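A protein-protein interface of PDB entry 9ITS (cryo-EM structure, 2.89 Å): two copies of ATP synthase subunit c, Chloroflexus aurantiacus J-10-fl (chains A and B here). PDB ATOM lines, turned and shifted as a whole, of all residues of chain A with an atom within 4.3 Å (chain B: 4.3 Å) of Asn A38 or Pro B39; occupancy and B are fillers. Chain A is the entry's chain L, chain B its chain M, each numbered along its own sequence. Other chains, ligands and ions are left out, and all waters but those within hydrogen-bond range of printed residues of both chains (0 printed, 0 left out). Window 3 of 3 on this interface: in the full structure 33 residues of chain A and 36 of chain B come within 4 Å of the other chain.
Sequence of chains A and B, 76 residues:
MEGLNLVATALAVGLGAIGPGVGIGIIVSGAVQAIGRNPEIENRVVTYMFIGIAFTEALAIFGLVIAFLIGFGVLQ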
ATOM      1  N   ALA A  34     -19.300  28.019  12.335  1.00  0.00           N
ATOM      2  CA  ALA A  34     -19.014  26.642  11.957  1.00  0.00           C
ATOM      3  C   ALA A  34     -18.739  26.483  10.469  1.00  0.00           C
ATOM      4  O   ALA A  34     -18.256  25.427  10.052  1.00  0.00           O
ATOM      5  CB  ALA A  34     -20.178  25.739  12.355  1.00  0.00           C
ATOM      6  N   GLY A  36     -16.911  28.988   8.959  1.00  0.00           N
ATOM      7  CA  GLY A  36     -15.571  29.542   8.847  1.00  0.00           C
ATOM      8  C   GLY A  36     -14.497  28.474   8.920  1.00  0.00           C
ATOM      9  O   GLY A  36     -13.465  28.571   8.252  1.00  0.00           O
ATOM     10  N   ARG A  37     -14.722  27.445   9.730  1.00  0.00           N
ATOM     11  CA  ARG A  37     -13.819  26.309   9.848  1.00  0.00           C
ATOM     12  C   ARG A  37     -14.499  25.074   9.275  1.00  0.00           C
ATOM     13  O   ARG A  37     -15.648  24.784   9.619  1.00  0.00           O
ATOM     14  CB  ARG A  37     -13.425  26.066  11.305  1.00  0.00           C
ATOM     15  CG  ARG A  37     -12.752  27.251  11.973  1.00  0.00           C
ATOM     16  CD  ARG A  37     -12.753  27.100  13.483  1.00  0.00           C
ATOM     17  NE  ARG A  37     -12.390  25.750  13.892  1.00  0.00           N
ATOM     18  CZ  ARG A  37     -11.560  25.466  14.886  1.00  0.00           C
ATOM     19  NH1 ARG A  37     -10.983  26.420  15.597  1.00  0.00           N
ATOM     20  NH2 ARG A  37     -11.302  24.194  15.174  1.00  0.00           N
ATOM     21  N   ASN A  38     -13.784  24.353   8.409  1.00  0.00           N
ATOM     22  CA  ASN A  38     -14.292  23.194   7.679  1.00  0.00           C
ATOM     23  C   ASN A  38     -15.531  23.544   6.859  1.00  0.00           C
ATOM     24  O   ASN A  38     -16.637  23.100   7.195  1.00  0.00           O
ATOM     25  CB  ASN A  38     -14.612  22.041   8.635  1.00  0.00           C
ATOM     26  CG  ASN A  38     -13.371  21.347   9.147  1.00  0.00           C
ATOM     27  OD1 ASN A  38     -12.387  21.193   8.425  1.00  0.00           O
ATOM     28  ND2 ASN A  38     -13.408  20.924  10.405  1.00  0.00           N
ATOM     29  N   PRO A  39     -15.398  24.330   5.785  1.00  0.00           N
ATOM     30  CA  PRO A  39     -16.556  24.603   4.921  1.00  0.00           C
ATOM     31  C   PRO A  39     -17.025  23.405   4.110  1.00  0.00           C
ATOM     32  O   PRO A  39     -18.053  23.510   3.433  1.00  0.00           O
ATOM     33  CB  PRO A  39     -16.050  25.722   3.997  1.00  0.00           C
ATOM     34  CG  PRO A  39     -14.857  26.292   4.688  1.00  0.00           C
ATOM     35  CD  PRO A  39     -14.234  25.136   5.392  1.00  0.00           C
ATOM     36  N   GLU A  40     -16.309  22.278   4.134  1.00  0.00           N
ATOM     37  CA  GLU A  40     -16.802  21.071   3.483  1.00  0.00           C
ATOM     38  C   GLU A  40     -17.991  20.461   4.213  1.00  0.00           C
ATOM     39  O   GLU A  40     -18.673  19.603   3.641  1.00  0.00           O
ATOM     40  CB  GLU A  40     -15.681  20.039   3.363  1.00  0.00           C
ATOM     41  CG  GLU A  40     -14.640  20.375   2.310  1.00  0.00           C
ATOM     42  CD  GLU A  40     -14.064  19.138   1.650  1.00  0.00           C
ATOM     43  OE1 GLU A  40     -14.363  18.021   2.120  1.00  0.00           O
ATOM     44  OE2 GLU A  40     -13.318  19.283   0.659  1.00  0.00           O
ATOM     45  N   ILE A  41     -18.246  20.874   5.454  1.00  0.00           N
ATOM     46  CA  ILE A  41     -19.471  20.533   6.167  1.00  0.00           C
ATOM     47  C   ILE A  41     -20.566  21.560   5.862  1.00  0.00           C
ATOM     48  O   ILE A  41     -21.660  21.512   6.438  1.00  0.00           O
ATOM     49  CB  ILE A  41     -19.171  20.405   7.676  1.00  0.00           C
ATOM     50  CG1 ILE A  41     -18.099  19.338   7.884  1.00  0.00           C
ATOM     51  CG2 ILE A  41     -20.346  19.872   8.488  1.00  0.00           C
ATOM     52  CD1 ILE A  41     -18.504  17.958   7.405  1.00  0.00           C
ATOM     53  N   ILE B  35     -20.035  20.414  15.541  1.00  0.00           N
ATOM     54  CA  ILE B  35     -19.889  19.657  14.301  1.00  0.00           C
ATOM     55  C   ILE B  35     -18.810  20.277  13.421  1.00  0.00           C
ATOM     56  O   ILE B  35     -18.003  19.566  12.811  1.00  0.00           O
ATOM     57  CB  ILE B  35     -21.242  19.562  13.570  1.00  0.00           C
ATOM     58  CG1 ILE B  35     -22.197  18.645  14.335  1.00  0.00           C
ATOM     59  CG2 ILE B  35     -21.056  19.029  12.159  1.00  0.00           C
ATOM     60  CD1 ILE B  35     -23.646  18.803  13.931  1.00  0.00           C
ATOM     61  N   GLY B  36     -18.770  21.608  13.348  1.00  0.00           N
ATOM     62  CA  GLY B  36     -17.742  22.268  12.559  1.00  0.00           C
ATOM     63  C   GLY B  36     -16.346  22.023  13.098  1.00  0.00           C
ATOM     64  O   GLY B  36     -15.391  21.878  12.329  1.00  0.00           O
ATOM     65  N   ARG B  37     -16.203  21.980  14.424  1.00  0.00           N
ATOM     66  CA  ARG B  37     -14.909  21.633  15.002  1.00  0.00           C
ATOM     67  C   ARG B  37     -14.610  20.147  14.832  1.00  0.00           C
ATOM     68  O   ARG B  37     -13.495  19.767  14.456  1.00  0.00           O
ATOM     69  CB  ARG B  37     -14.862  22.029  16.478  1.00  0.00           C
ATOM     70  CG  ARG B  37     -14.750  23.526  16.711  1.00  0.00           C
ATOM     71  CD  ARG B  37     -14.712  23.859  18.194  1.00  0.00           C
ATOM     72  NE  ARG B  37     -13.437  23.497  18.802  1.00  0.00           N
ATOM     73  CZ  ARG B  37     -13.255  22.451  19.596  1.00  0.00           C
ATOM     74  NH1 ARG B  37     -14.249  21.634  19.902  1.00  0.00           N
ATOM     75  NH2 ARG B  37     -12.044  22.217  20.095  1.00  0.00           N
ATOM     76  N   ASN B  38     -15.597  19.290  15.095  1.00  0.00           N
ATOM     77  CA  ASN B  38     -15.413  17.838  15.071  1.00  0.00           C
ATOM     78  C   ASN B  38     -16.507  17.192  14.232  1.00  0.00           C
ATOM     79  O   ASN B  38     -17.525  16.732  14.767  1.00  0.00           O
ATOM     80  CB  ASN B  38     -15.406  17.268  16.488  1.00  0.00           C
ATOM     81  CG  ASN B  38     -14.898  15.843  16.539  1.00  0.00           C
ATOM     82  OD1 ASN B  38     -14.443  15.296  15.536  1.00  0.00           O
ATOM     83  ND2 ASN B  38     -14.973  15.232  17.716  1.00  0.00           N
ATOM     84  N   PRO B  39     -16.335  17.144  12.907  1.00  0.00           N
ATOM     85  CA  PRO B  39     -17.360  16.508  12.060  1.00  0.00           C
ATOM     86  C   PRO B  39     -17.514  15.014  12.298  1.00  0.00           C
ATOM     87  O   PRO B  39     -18.559  14.452  11.949  1.00  0.00           O
ATOM     88  CB  PRO B  39     -16.873  16.803  10.634  1.00  0.00           C
ATOM     89  CG  PRO B  39     -15.915  17.946  10.776  1.00  0.00           C
ATOM     90  CD  PRO B  39     -15.267  17.766  12.109  1.00  0.00           C
ATOM     91  N   GLU B  40     -16.508  14.355  12.875  1.00  0.00           N
ATOM     92  CA  GLU B  40     -16.587  12.911  13.078  1.00  0.00           C
ATOM     93  C   GLU B  40     -17.604  12.541  14.152  1.00  0.00           C
ATOM     94  O   GLU B  40     -18.201  11.460  14.091  1.00  0.00           O
ATOM     95  CB  GLU B  40     -15.206  12.362  13.439  1.00  0.00           C
ATOM     96  CG  GLU B  40     -15.063  10.860  13.273  1.00  0.00           C
ATOM     97  CD  GLU B  40     -15.270  10.110  14.574  1.00  0.00           C
ATOM     98  OE1 GLU B  40     -15.130  10.733  15.647  1.00  0.00           O
ATOM     99  OE2 GLU B  40     -15.573   8.899  14.523  1.00  0.00           O
ATOM    100  N   ILE B  41     -17.819  13.422  15.136  1.00  0.00           N
ATOM    101  CA  ILE B  41     -18.723  13.132  16.245  1.00  0.00           C
ATOM    102  C   ILE B  41     -20.151  13.598  15.974  1.00  0.00           C
ATOM    103  O   ILE B  41     -20.999  13.535  16.876  1.00  0.00           O
ATOM    104  CB  ILE B  41     -18.150  13.756  17.538  1.00  0.00           C
ATOM    105  CG1 ILE B  41     -18.585  12.967  18.778  1.00  0.00           C
ATOM    106  CG2 ILE B  41     -18.496  15.242  17.637  1.00  0.00           C
ATOM    107  CD1 ILE B  41     -18.089  11.537  18.796  1.00  0.00           C
ATOM    108  N   GLU B  42     -20.453  14.018  14.741  1.00  0.00           N
ATOM    109  CA  GLU B  42     -21.747  14.624  14.433  1.00  0.00           C
ATOM    110  C   GLU B  42     -22.906  13.664  14.688  1.00  0.00           C
ATOM    111  O   GLU B  42     -23.962  14.074  15.191  1.00  0.00           O
ATOM    112  CB  GLU B  42     -21.751  15.103  12.980  1.00  0.00           C
ATOM    113  CG  GLU B  42     -23.126  15.260  12.361  1.00  0.00           C
ATOM    114  CD  GLU B  42     -23.061  15.717  10.919  1.00  0.00           C
ATOM    115  OE1 GLU B  42     -21.977  16.159  10.483  1.00  0.00           O
ATOM    116  OE2 GLU B  42     -24.091  15.630  10.219  1.00  0.00           O
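Of the 7 printed residues of chain A, 3 touch a printed residue of chain B.
Hydrophobic or aromatic side chains of chain A within 4 Å of the printed part of chain B: Ile A41.
Printed residues of chain B that touch a printed residue of chain A: Ile B35, Gly B36, Arg B37 and Pro B39.
Hydrophobic or aromatic side chains of chain B that line the printed part of chain A: Ile B35 and Pro B39.
Among the printed residues, 6 pairs touch across the chains.
Among the printed residues, no Asp or Glu carboxylate lies within 4 Å of a Lys or Arg side-chain nitrogen of the other chain.
ND2 of Asn A38 is in hydrogen-bond range of O of Gly B36, at 2.9 Å.
Asn A38 touches just these residues of chain B: Gly B36 (2.9 Å) and Pro B39 (3.9 Å).
Pro B39 touches two residues of chain A.
Of the printed residues of chain A, Arg B37 touches Arg A37 (3.8 Å).
Printed residues of chain A within 4 Å of Ile B35: Ile A41.
Asn B38 touches none of the printed residues of chain A.
The nearest residue of chain B that does not touch Asn A38 is Arg B37 (4.2 Å).
The nearest printed residue of chain A that does not touch Arg B37 is Asn A38 (4.2 Å).
Arg A37 touches Gly B36, but with the chains exchanged Gly A36 does not touch Arg B37 (8.7 Å).
Arg A37 touches its own counterpart, Arg B37.
Asn A38 touches Gly B36, but with the chains exchanged Gly A36 does not touch Asn B38 (11.1 Å).
Asn A38 touches Pro B39, but with the chains exchanged Pro A39 does not touch Asn B38 (10.6 Å).
Positions printed for both chains: 36, 37, 38, 39, 40 and 41.
Of the 6 pairs that touch across the chains among the printed residues, 1 has its exchanged pair printed and touching as well.
Among the printed residues, pairs that only touch across the chains: Ile A41 with Pro B39 (3.8 Å), Ile A41 with Ile B35 (3.8 Å), Arg A37 with Arg B37 (3.8 Å), Asn A38 with Pro B39 (3.9 Å) and Arg A37 with Gly B36 (3.98 Å).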
